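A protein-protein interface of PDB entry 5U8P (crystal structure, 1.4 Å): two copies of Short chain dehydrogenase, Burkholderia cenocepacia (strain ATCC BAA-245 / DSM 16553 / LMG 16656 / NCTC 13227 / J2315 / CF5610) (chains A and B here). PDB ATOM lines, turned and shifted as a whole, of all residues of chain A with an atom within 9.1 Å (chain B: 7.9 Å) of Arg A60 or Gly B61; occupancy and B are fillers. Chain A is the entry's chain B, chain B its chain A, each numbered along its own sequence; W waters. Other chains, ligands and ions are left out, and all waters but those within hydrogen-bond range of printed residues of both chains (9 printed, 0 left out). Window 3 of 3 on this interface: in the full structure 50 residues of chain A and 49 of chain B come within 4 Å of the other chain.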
ATOM      1  N   GLY A  19      12.610  19.113  11.096  1.00  0.00           N
ATOM      2  CA  GLY A  19      11.481  20.016  11.012  1.00  0.00           C
ATOM      3  C   GLY A  19      11.882  21.472  10.878  1.00  0.00           C
ATOM      4  O   GLY A  19      13.060  21.829  10.981  1.00  0.00           O
ATOM      5  N   SER A  56      23.804  21.538  20.345  1.00  0.00           N
ATOM      6  CA  SER A  56      22.978  21.384  19.157  1.00  0.00           C
ATOM      7  C   SER A  56      23.695  20.787  17.957  1.00  0.00           C
ATOM      8  O   SER A  56      23.024  20.223  17.085  1.00  0.00           O
ATOM      9  CB  SER A  56      22.387  22.727  18.733  1.00  0.00           C
ATOM     10  OG  SER A  56      23.423  23.648  18.416  1.00  0.00           O
ATOM     11  N   TYR A  57      25.015  20.928  17.837  1.00  0.00           N
ATOM     12  CA  TYR A  57      25.665  20.531  16.589  1.00  0.00           C
ATOM     13  C   TYR A  57      25.837  19.017  16.543  1.00  0.00           C
ATOM     14  O   TYR A  57      26.519  18.442  17.392  1.00  0.00           O
ATOM     15  CB  TYR A  57      27.005  21.245  16.360  1.00  0.00           C
ATOM     16  CG  TYR A  57      27.442  21.023  14.928  1.00  0.00           C
ATOM     17  CD1 TYR A  57      28.143  19.877  14.564  1.00  0.00           C
ATOM     18  CD2 TYR A  57      27.085  21.916  13.934  1.00  0.00           C
ATOM     19  CE1 TYR A  57      28.492  19.627  13.238  1.00  0.00           C
ATOM     20  CE2 TYR A  57      27.437  21.690  12.613  1.00  0.00           C
ATOM     21  CZ  TYR A  57      28.135  20.544  12.265  1.00  0.00           C
ATOM     22  OH  TYR A  57      28.475  20.340  10.946  1.00  0.00           O
ATOM     23  N   ARG A  58      25.245  18.371  15.538  1.00  0.00           N
ATOM     24  CA  ARG A  58      25.376  16.931  15.349  1.00  0.00           C
ATOM     25  C   ARG A  58      26.136  16.678  14.053  1.00  0.00           C
ATOM     26  O   ARG A  58      25.710  17.118  12.979  1.00  0.00           O
ATOM     27  CB  ARG A  58      24.005  16.251  15.309  1.00  0.00           C
ATOM     28  N   GLY A  59      27.256  15.973  14.161  1.00  0.00           N
ATOM     29  CA  GLY A  59      28.041  15.636  12.999  1.00  0.00           C
ATOM     30  C   GLY A  59      27.432  14.509  12.175  1.00  0.00           C
ATOM     31  O   GLY A  59      26.601  13.722  12.630  1.00  0.00           O
ATOM     32  N   ARG A  60      27.878  14.439  10.921  1.00  0.00           N
ATOM     33  CA  ARG A  60      27.384  13.465   9.956  1.00  0.00           C
ATOM     34  C   ARG A  60      28.518  12.943   9.078  1.00  0.00           C
ATOM     35  O   ARG A  60      28.304  12.639   7.898  1.00  0.00           O
ATOM     36  CB  ARG A  60      26.291  14.071   9.060  1.00  0.00           C
ATOM     37  CG  ARG A  60      25.348  15.030   9.761  1.00  0.00           C
ATOM     38  CD  ARG A  60      24.476  15.780   8.779  1.00  0.00           C
ATOM     39  NE  ARG A  60      23.686  16.778   9.485  1.00  0.00           N
ATOM     40  CZ  ARG A  60      22.432  16.599   9.874  1.00  0.00           C
ATOM     41  NH1 ARG A  60      21.791  17.567  10.523  1.00  0.00           N
ATOM     42  NH2 ARG A  60      21.819  15.455   9.611  1.00  0.00           N
ATOM     43  N   GLY A  61      29.730  12.862   9.623  1.00  0.00           N
ATOM     44  CA  GLY A  61      30.852  12.278   8.900  1.00  0.00           C
ATOM     45  C   GLY A  61      31.318  13.065   7.699  1.00  0.00           C
ATOM     46  O   GLY A  61      31.758  12.466   6.713  1.00  0.00           O
ATOM     47  N   ARG A  62      31.251  14.399   7.754  1.00  0.00           N
ATOM     48  CA  ARG A  62      31.551  15.211   6.585  1.00  0.00           C
ATOM     49  C   ARG A  62      33.028  15.549   6.424  1.00  0.00           C
ATOM     50  O   ARG A  62      33.413  16.030   5.353  1.00  0.00           O
ATOM     51  CB  ARG A  62      30.701  16.495   6.593  1.00  0.00           C
ATOM     52  CG  ARG A  62      29.209  16.176   6.432  1.00  0.00           C
ATOM     53  CD  ARG A  62      28.318  17.380   6.648  1.00  0.00           C
ATOM     54  NE  ARG A  62      28.553  18.435   5.654  1.00  0.00           N
ATOM     55  CZ  ARG A  62      28.131  19.693   5.797  1.00  0.00           C
ATOM     56  NH1 ARG A  62      27.452  20.055   6.880  1.00  0.00           N
ATOM     57  NH2 ARG A  62      28.415  20.602   4.873  1.00  0.00           N
ATOM     58  N   LEU A  63      33.851  15.329   7.454  1.00  0.00           N
ATOM     59  CA  LEU A  63      35.264  15.727   7.450  1.00  0.00           C
ATOM     60  C   LEU A  63      36.134  14.666   8.125  1.00  0.00           C
ATOM     61  O   LEU A  63      37.091  14.987   8.841  1.00  0.00           O
ATOM     62  CB  LEU A  63      35.459  17.082   8.146  1.00  0.00           C
ATOM     63  CG  LEU A  63      34.754  18.307   7.550  1.00  0.00           C
ATOM     64  CD1 LEU A  63      34.891  19.479   8.507  1.00  0.00           C
ATOM     65  CD2 LEU A  63      35.339  18.684   6.192  1.00  0.00           C
ATOM     66  N   VAL A  64      35.832  13.385   7.885  1.00  0.00           N
ATOM     67  CA  VAL A  64      36.490  12.315   8.638  1.00  0.00           C
ATOM     68  C   VAL A  64      37.985  12.280   8.349  1.00  0.00           C
ATOM     69  O   VAL A  64      38.414  12.195   7.191  1.00  0.00           O
ATOM     70  CB  VAL A  64      35.835  10.956   8.341  1.00  0.00           C
ATOM     71  CG1 VAL A  64      36.588   9.835   9.070  1.00  0.00           C
ATOM     72  CG2 VAL A  64      34.362  10.963   8.758  1.00  0.00           C
ATOM     73  N   ALA A  84      32.290  21.907  15.548  1.00  0.00           N
ATOM     74  CA  ALA A  84      31.674  21.287  14.376  1.00  0.00           C
ATOM     75  C   ALA A  84      32.670  20.407  13.626  1.00  0.00           C
ATOM     76  O   ALA A  84      32.337  19.281  13.226  1.00  0.00           O
ATOM     77  CB  ALA A  84      31.081  22.366  13.461  1.00  0.00           C
ATOM     78  N   PHE A  85      33.893  20.909  13.399  1.00  0.00           N
ATOM     79  CA  PHE A  85      34.907  20.111  12.702  1.00  0.00           C
ATOM     80  C   PHE A  85      35.130  18.784  13.419  1.00  0.00           C
ATOM     81  O   PHE A  85      35.172  17.724  12.783  1.00  0.00           O
ATOM     82  CB  PHE A  85      36.240  20.861  12.618  1.00  0.00           C
ATOM     83  CG  PHE A  85      36.280  22.023  11.644  1.00  0.00           C
ATOM     84  CD1 PHE A  85      35.376  22.179  10.618  1.00  0.00           C
ATOM     85  CD2 PHE A  85      37.276  22.964  11.786  1.00  0.00           C
ATOM     86  CE1 PHE A  85      35.477  23.274   9.738  1.00  0.00           C
ATOM     87  CE2 PHE A  85      37.371  24.050  10.924  1.00  0.00           C
ATOM     88  CZ  PHE A  85      36.485  24.182   9.889  1.00  0.00           C
ATOM     89  N   ALA A  86      35.281  18.825  14.746  1.00  0.00           N
ATOM     90  CA  ALA A  86      35.533  17.594  15.493  1.00  0.00           C
ATOM     91  C   ALA A  86      34.360  16.635  15.370  1.00  0.00           C
ATOM     92  O   ALA A  86      34.553  15.429  15.165  1.00  0.00           O
ATOM     93  CB  ALA A  86      35.788  17.929  16.962  1.00  0.00           C
ATOM     94  N   ARG A  87      33.135  17.159  15.456  1.00  0.00           N
ATOM     95  CA  ARG A  87      31.956  16.314  15.354  1.00  0.00           C
ATOM     96  C   ARG A  87      31.772  15.746  13.959  1.00  0.00           C
ATOM     97  O   ARG A  87      31.111  14.715  13.813  1.00  0.00           O
ATOM     98  CB  ARG A  87      30.725  17.051  15.870  1.00  0.00           C
ATOM     99  CG  ARG A  87      30.821  17.202  17.374  1.00  0.00           C
ATOM    100  CD  ARG A  87      29.572  17.735  17.992  1.00  0.00           C
ATOM    101  NE  ARG A  87      29.807  17.956  19.413  1.00  0.00           N
ATOM    102  CZ  ARG A  87      29.080  18.779  20.144  1.00  0.00           C
ATOM    103  NH1 ARG A  87      28.064  19.421  19.575  1.00  0.00           N
ATOM    104  NH2 ARG A  87      29.394  18.993  21.416  1.00  0.00           N
ATOM    105  N   GLU A  88      32.329  16.401  12.942  1.00  0.00           N
ATOM    106  CA  GLU A  88      32.342  15.862  11.589  1.00  0.00           C
ATOM    107  C   GLU A  88      33.498  14.898  11.349  1.00  0.00           C
ATOM    108  O   GLU A  88      33.644  14.409  10.219  1.00  0.00           O
ATOM    109  CB  GLU A  88      32.387  17.010  10.570  1.00  0.00           C
ATOM    110  CG  GLU A  88      31.152  17.932  10.576  1.00  0.00           C
ATOM    111  CD  GLU A  88      29.860  17.225  10.187  1.00  0.00           C
ATOM    112  OE1 GLU A  88      29.893  16.044   9.755  1.00  0.00           O
ATOM    113  OE2 GLU A  88      28.789  17.868  10.309  1.00  0.00           O
ATOM    114  N   GLY A  89      34.300  14.606  12.376  1.00  0.00           N
ATOM    115  CA  GLY A  89      35.347  13.605  12.290  1.00  0.00           C
ATOM    116  C   GLY A  89      36.761  14.113  12.097  1.00  0.00           C
ATOM    117  O   GLY A  89      37.659  13.293  11.848  1.00  0.00           O
ATOM    118  N   PRO A 283      28.126  26.001  10.220  1.00  0.00           N
ATOM    119  CA  PRO A 283      27.877  25.310   8.946  1.00  0.00           C
ATOM    120  C   PRO A 283      28.620  25.896   7.755  1.00  0.00           C
ATOM    121  O   PRO A 283      28.898  25.155   6.805  1.00  0.00           O
ATOM    122  CB  PRO A 283      26.350  25.392   8.791  1.00  0.00           C
ATOM    123  CG  PRO A 283      25.846  25.420  10.217  1.00  0.00           C
ATOM    124  CD  PRO A 283      26.849  26.305  10.912  1.00  0.00           C
ATOM    125  N   VAL A 286      32.142  24.293   7.815  1.00  0.00           N
ATOM    126  CA  VAL A 286      32.092  22.886   7.403  1.00  0.00           C
ATOM    127  C   VAL A 286      31.896  22.777   5.896  1.00  0.00           C
ATOM    128  O   VAL A 286      32.594  22.012   5.216  1.00  0.00           O
ATOM    129  CB  VAL A 286      31.009  22.116   8.184  1.00  0.00           C
ATOM    130  CG1 VAL A 286      30.921  20.667   7.682  1.00  0.00           C
ATOM    131  CG2 VAL A 286      31.294  22.150   9.690  1.00  0.00           C
ATOM    132  N   TYR B  57      26.710  12.077  -5.220  1.00  0.00           N
ATOM    133  CA  TYR B  57      26.120  12.806  -4.098  1.00  0.00           C
ATOM    134  C   TYR B  57      25.510  11.821  -3.101  1.00  0.00           C
ATOM    135  O   TYR B  57      24.601  11.071  -3.450  1.00  0.00           O
ATOM    136  CB  TYR B  57      25.080  13.847  -4.535  1.00  0.00           C
ATOM    137  CG  TYR B  57      24.739  14.732  -3.339  1.00  0.00           C
ATOM    138  CD1 TYR B  57      23.767  14.355  -2.416  1.00  0.00           C
ATOM    139  CD2 TYR B  57      25.442  15.912  -3.109  1.00  0.00           C
ATOM    140  CE1 TYR B  57      23.500  15.129  -1.292  1.00  0.00           C
ATOM    141  CE2 TYR B  57      25.182  16.696  -1.995  1.00  0.00           C
ATOM    142  CZ  TYR B  57      24.212  16.297  -1.085  1.00  0.00           C
ATOM    143  OH  TYR B  57      23.969  17.101   0.016  1.00  0.00           O
ATOM    144  N   ARG B  58      25.978  11.855  -1.855  1.00  0.00           N
ATOM    145  CA  ARG B  58      25.457  10.997  -0.795  1.00  0.00           C
ATOM    146  C   ARG B  58      24.751  11.870   0.235  1.00  0.00           C
ATOM    147  O   ARG B  58      25.354  12.798   0.791  1.00  0.00           O
ATOM    148  CB  ARG B  58      26.566  10.165  -0.141  1.00  0.00           C
ATOM    149  N   GLY B  59      23.470  11.596   0.460  1.00  0.00           N
ATOM    150  CA  GLY B  59      22.719  12.321   1.465  1.00  0.00           C
ATOM    151  C   GLY B  59      23.036  11.879   2.890  1.00  0.00           C
ATOM    152  O   GLY B  59      23.535  10.781   3.161  1.00  0.00           O
ATOM    153  N   ARG B  60      22.730  12.778   3.834  1.00  0.00           N
ATOM    154  CA  ARG B  60      23.042  12.585   5.245  1.00  0.00           C
ATOM    155  C   ARG B  60      21.905  13.075   6.129  1.00  0.00           C
ATOM    156  O   ARG B  60      22.146  13.522   7.256  1.00  0.00           O
ATOM    157  CB  ARG B  60      24.332  13.320   5.637  1.00  0.00           C
ATOM    158  CG  ARG B  60      25.484  13.096   4.682  1.00  0.00           C
ATOM    159  CD  ARG B  60      26.641  14.010   4.989  1.00  0.00           C
ATOM    160  NE  ARG B  60      27.582  14.005   3.880  1.00  0.00           N
ATOM    161  CZ  ARG B  60      28.674  13.257   3.828  1.00  0.00           C
ATOM    162  NH1 ARG B  60      28.985  12.459   4.842  1.00  0.00           N
ATOM    163  NH2 ARG B  60      29.463  13.322   2.758  1.00  0.00           N
ATOM    164  N   GLY B  61      20.676  13.039   5.619  1.00  0.00           N
ATOM    165  CA  GLY B  61      19.516  13.415   6.406  1.00  0.00           C
ATOM    166  C   GLY B  61      19.433  14.883   6.770  1.00  0.00           C
ATOM    167  O   GLY B  61      18.922  15.223   7.846  1.00  0.00           O
ATOM    168  N   ARG B  62      19.915  15.777   5.901  1.00  0.00           N
ATOM    169  CA  ARG B  62      20.004  17.189   6.255  1.00  0.00           C
ATOM    170  C   ARG B  62      18.732  17.976   5.984  1.00  0.00           C
ATOM    171  O   ARG B  62      18.619  19.097   6.482  1.00  0.00           O
ATOM    172  CB  ARG B  62      21.206  17.853   5.557  1.00  0.00           C
ATOM    173  CG  ARG B  62      22.538  17.273   6.057  1.00  0.00           C
ATOM    174  CD  ARG B  62      23.718  17.683   5.195  1.00  0.00           C
ATOM    175  NE  ARG B  62      23.938  19.134   5.264  1.00  0.00           N
ATOM    176  CZ  ARG B  62      24.704  19.807   4.405  1.00  0.00           C
ATOM    177  NH1 ARG B  62      25.323  19.160   3.409  1.00  0.00           N
ATOM    178  NH2 ARG B  62      24.829  21.129   4.518  1.00  0.00           N
ATOM    179  N   LEU B  63      17.773  17.418   5.239  1.00  0.00           N
ATOM    180  CA  LEU B  63      16.562  18.136   4.831  1.00  0.00           C
ATOM    181  C   LEU B  63      15.338  17.222   4.899  1.00  0.00           C
ATOM    182  O   LEU B  63      14.447  17.285   4.043  1.00  0.00           O
ATOM    183  CB  LEU B  63      16.711  18.716   3.421  1.00  0.00           C
ATOM    184  CG  LEU B  63      17.838  19.725   3.172  1.00  0.00           C
ATOM    185  CD1 LEU B  63      17.991  19.994   1.672  1.00  0.00           C
ATOM    186  CD2 LEU B  63      17.588  21.040   3.911  1.00  0.00           C
ATOM    187  N   VAL B  64      15.270  16.362   5.922  1.00  0.00           N
ATOM    188  CA  VAL B  64      14.238  15.324   5.951  1.00  0.00           C
ATOM    189  C   VAL B  64      12.850  15.945   6.020  1.00  0.00           C
ATOM    190  O   VAL B  64      12.546  16.750   6.911  1.00  0.00           O
ATOM    191  CB  VAL B  64      14.472  14.350   7.117  1.00  0.00           C
ATOM    192  CG1 VAL B  64      13.364  13.306   7.146  1.00  0.00           C
ATOM    193  CG2 VAL B  64      15.835  13.669   6.992  1.00  0.00           C
ATOM    194  N   GLY B  65      11.989  15.547   5.089  1.00  0.00           N
ATOM    195  CA  GLY B  65      10.619  16.007   5.086  1.00  0.00           C
ATOM    196  C   GLY B  65      10.405  17.394   4.527  1.00  0.00           C
ATOM    197  O   GLY B  65       9.264  17.882   4.544  1.00  0.00           O
ATOM    198  N   ALA B  84      20.354  16.453  -4.911  1.00  0.00           N
ATOM    199  CA  ALA B  84      20.868  16.564  -3.550  1.00  0.00           C
ATOM    200  C   ALA B  84      19.733  16.728  -2.546  1.00  0.00           C
ATOM    201  O   ALA B  84      19.739  16.091  -1.481  1.00  0.00           O
ATOM    202  CB  ALA B  84      21.881  17.714  -3.469  1.00  0.00           C
ATOM    203  N   ALA B  86      16.616  15.678  -2.775  1.00  0.00           N
ATOM    204  CA  ALA B  86      15.946  14.390  -2.590  1.00  0.00           C
ATOM    205  C   ALA B  86      16.790  13.450  -1.732  1.00  0.00           C
ATOM    206  O   ALA B  86      16.270  12.786  -0.822  1.00  0.00           O
ATOM    207  CB  ALA B  86      15.631  13.752  -3.946  1.00  0.00           C
ATOM    208  N   ARG B  87      18.101  13.390  -1.992  1.00  0.00           N
ATOM    209  CA  ARG B  87      18.950  12.501  -1.210  1.00  0.00           C
ATOM    210  C   ARG B  87      19.109  12.941   0.238  1.00  0.00           C
ATOM    211  O   ARG B  87      19.419  12.095   1.082  1.00  0.00           O
ATOM    212  CB  ARG B  87      20.288  12.303  -1.906  1.00  0.00           C
ATOM    213  CG  ARG B  87      20.091  11.488  -3.160  1.00  0.00           C
ATOM    214  CD  ARG B  87      21.388  11.134  -3.844  1.00  0.00           C
ATOM    215  NE  ARG B  87      21.097  10.459  -5.108  1.00  0.00           N
ATOM    216  CZ  ARG B  87      21.968  10.343  -6.097  1.00  0.00           C
ATOM    217  NH1 ARG B  87      23.199  10.821  -5.935  1.00  0.00           N
ATOM    218  NH2 ARG B  87      21.606   9.774  -7.241  1.00  0.00           N
ATOM    219  N   GLU B  88      18.886  14.219   0.544  1.00  0.00           N
ATOM    220  CA  GLU B  88      18.879  14.715   1.920  1.00  0.00           C
ATOM    221  C   GLU B  88      17.524  14.543   2.592  1.00  0.00           C
ATOM    222  O   GLU B  88      17.361  14.960   3.742  1.00  0.00           O
ATOM    223  CB  GLU B  88      19.313  16.199   1.956  1.00  0.00           C
ATOM    224  CG  GLU B  88      20.756  16.461   1.515  1.00  0.00           C
ATOM    225  CD  GLU B  88      21.805  15.798   2.413  1.00  0.00           C
ATOM    226  OE1 GLU B  88      21.465  15.253   3.495  1.00  0.00           O
ATOM    227  OE2 GLU B  88      22.996  15.830   2.040  1.00  0.00           O
ATOM    228  N   GLY B  89      16.560  13.924   1.910  1.00  0.00           N
ATOM    229  CA  GLY B  89      15.288  13.597   2.512  1.00  0.00           C
ATOM    230  C   GLY B  89      14.121  14.480   2.139  1.00  0.00           C
ATOM    231  O   GLY B  89      13.047  14.322   2.736  1.00  0.00           O
ATOM    232  N   ALA B  90      14.278  15.386   1.166  1.00  0.00           N
ATOM    233  CA  ALA B  90      13.212  16.308   0.785  1.00  0.00           C
ATOM    234  C   ALA B  90      12.414  15.770  -0.398  1.00  0.00           C
ATOM    235  O   ALA B  90      12.953  15.098  -1.282  1.00  0.00           O
ATOM    236  CB  ALA B  90      13.784  17.681   0.407  1.00  0.00           C
ATOM    237  N   VAL B 286      22.091  22.990  -0.523  1.00  0.00           N
ATOM    238  CA  VAL B 286      21.770  22.243   0.695  1.00  0.00           C
ATOM    239  C   VAL B 286      22.100  23.070   1.930  1.00  0.00           C
ATOM    240  O   VAL B 286      21.282  23.188   2.853  1.00  0.00           O
ATOM    241  CB  VAL B 286      22.491  20.881   0.707  1.00  0.00           C
ATOM    242  CG1 VAL B 286      22.227  20.150   2.017  1.00  0.00           C
ATOM    243  CG2 VAL B 286      22.040  20.030  -0.474  1.00  0.00           C
ATOM    244  N   ALA B 290      19.335  24.394   4.783  1.00  0.00           N
ATOM    245  CA  ALA B 290      19.292  23.667   6.053  1.00  0.00           C
ATOM    246  C   ALA B 290      18.876  24.574   7.208  1.00  0.00           C
ATOM    247  O   ALA B 290      19.295  25.733   7.305  1.00  0.00           O
ATOM    248  CB  ALA B 290      20.657  23.044   6.332  1.00  0.00           C
ATOM    249  N   SER B 291      18.082  24.018   8.126  1.00  0.00           N
ATOM    250  CA  SER B 291      17.581  24.800   9.255  1.00  0.00           C
ATOM    251  C   SER B 291      18.704  25.327  10.146  1.00  0.00           C
ATOM    252  O   SER B 291      18.543  26.373  10.793  1.00  0.00           O
ATOM    253  CB  SER B 291      16.597  23.967  10.076  1.00  0.00           C
ATOM    254  OG  SER B 291      15.490  23.554   9.285  1.00  0.00           O
ATOM    255  N   GLU B 292      19.838  24.623  10.207  1.00  0.00           N
ATOM    256  CA  GLU B 292      20.932  25.033  11.093  1.00  0.00           C
ATOM    257  C   GLU B 292      21.654  26.285  10.603  1.00  0.00           C
ATOM    258  O   GLU B 292      22.372  26.911  11.389  1.00  0.00           O
ATOM    259  CB  GLU B 292      21.952  23.902  11.267  1.00  0.00           C
ATOM    260  CG  GLU B 292      22.646  23.537   9.950  1.00  0.00           C
ATOM    261  CD  GLU B 292      23.789  22.554  10.113  1.00  0.00           C
ATOM    262  OE1 GLU B 292      24.096  22.117  11.255  1.00  0.00           O
ATOM    263  OE2 GLU B 292      24.386  22.216   9.063  1.00  0.00           O
HETATM  264  O   HOH W   1      13.988  18.545   8.393  1.00  0.00           O
HETATM  265  O   HOH W   2      27.131  22.068   9.049  1.00  0.00           O
HETATM  266  O   HOH W   3      26.685  21.805   2.314  1.00  0.00           O
HETATM  267  O   HOH W   4      19.406  17.561  10.225  1.00  0.00           O
HETATM  268  O   HOH W   5      20.575  19.739   8.418  1.00  0.00           O
HETATM  269  O   HOH W   6      27.138  23.074   5.878  1.00  0.00           O
HETATM  270  O   HOH W   7      32.016  12.837   3.311  1.00  0.00           O
HETATM  271  O   HOH W   8      24.683  19.443  11.127  1.00  0.00           O
HETATM  272  O   HOH W   9      31.498  15.794   3.212  1.00  0.00           O
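Tyr A57 touches Glu B292 (CE2 to OE1, 3.6 Å). Arg A60 touches Arg B62. Arg B60 touches Arg A62. Arg A62 touches Arg B62 (NH2 to NH2, 3.6 Å). Pro A283 touches Glu B292 (CG to CD, 3.5 Å).
NH1 of Arg B60 is in hydrogen-bond range of O of Gly A61. The backbone carbonyl oxygen of Gly B61 lies within hydrogen-bond range of the guanidinium group of Arg A60, 3.4 Å away. The backbone carbonyl oxygen of Arg B60 lies within hydrogen-bond range of the guanidinium group of Arg A60, at 3.1 Å. The side-chain hydroxyl of Ser B291 is in hydrogen-bond range of the backbone carbonyl oxygen of Gly A19 (3.4 Å).
The backbone NH of Arg A60 lies within hydrogen-bond range of the side-chain carboxylate of Glu A88 (2.8 Å). The backbone NH (N) of Gly B61 is in hydrogen-bond range of the side-chain carboxylate (OE1) of Glu B88, 3.2 Å away. The backbone NH (N) of Gly A61 is in hydrogen-bond range of the side-chain carboxylate (OE1) of Glu A88, at 3.2 Å. The backbone NH of Arg B60 sits at hydrogen-bond distance from the side-chain carboxylate of Glu B88 (2.8 Å). The backbone NH (N) of Arg B62 lies within hydrogen-bond range of the side-chain carboxylate (OE1) of Glu B88 (2.9 Å). O of Tyr A57 lies within hydrogen-bond range of NH1 of Arg A87 (2.8 Å).
Water W4 lies within hydrogen-bond range of NH1 of Arg A60 (2.4 Å) and O of Gly B61 (3.4 Å). Water W1 bridges O of Val B64 (2.7 Å) and N of Gly A19 (3.1 Å). Water W8 lies within hydrogen-bond range of the side-chain carboxylate (OE1) of Glu B292 (2.7 Å), the backbone carbonyl oxygen (O) of Arg A58 (3.1 Å) and the guanidinium group (NE) of Arg A60 (3.3 Å). Water W2 lies within hydrogen-bond range of OE2 of Glu B292 (2.7 Å), OH of Tyr A57 (2.9 Å) and NH1 of Arg A62 (3.0 Å). Water W5 bridges O of Arg B62 (2.8 Å) and NH1 of Arg A60 (3.3 Å). Water W9 lies within hydrogen-bond range of the backbone carbonyl oxygen (O) of Arg A62 (2.9 Å) and the guanidinium group (NH2) of Arg B60 (3.2 Å).
Hydrophobic or aromatic side chains of chain A that line the printed part of chain B: Tyr A57 and Pro A283. Along chain A the printed residues that touch a printed residue of chain B span positions 19 to 283. Of the 19 printed residues of chain B, 5 touch a printed residue of chain A. Among the printed residues, 9 pairs touch across the chains. Among the printed residues, no Asp or Glu carboxylate lies within 4 Å of a Lys or Arg side-chain nitrogen of the other chain.
Of the printed residues of chain B, Gly A19 touches Ser B291 (3.4 Å). Gly A59 touches none of the printed residues of chain B. Of chain B, only Arg B60 (3.1 Å), Gly B61 (3.4 Å) and Arg B62 (3.6 Å) come within 4 Å of Arg A60. Of chain B, only Arg B60 comes within 4 Å of Gly A61. Printed residues of chain B within 4 Å of Arg A62: Arg B60 and Arg B62. Ala A84 touches none of the printed residues of chain B. Of the printed residues of chain B, Pro A283 touches Glu B292. Of chain A, only Arg A60 (3.4 Å) comes within 4 Å of Gly B61. Val B64 touches none of the printed residues of chain A. Of the printed residues of chain A, Ser B291 touches Gly A19 (3.4 Å). The nearest residue of chain B that does not touch Arg A60 is Glu B292 (5.2 Å). The nearest printed residue of chain A that does not touch Ser B291 is Pro A283 (7.1 Å).
Arg B60 touches its own counterpart, Arg A60. Arg A60 touches Gly B61, and with the chains exchanged Gly A61 touches Arg B60. Arg A60 touches Arg B62, and with the chains exchanged Arg A62 touches Arg B60. Arg B62 touches its own counterpart, Arg A62. Of the 9 pairs that touch across the chains among the printed residues, 6 have their exchanged pair printed and touching as well.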
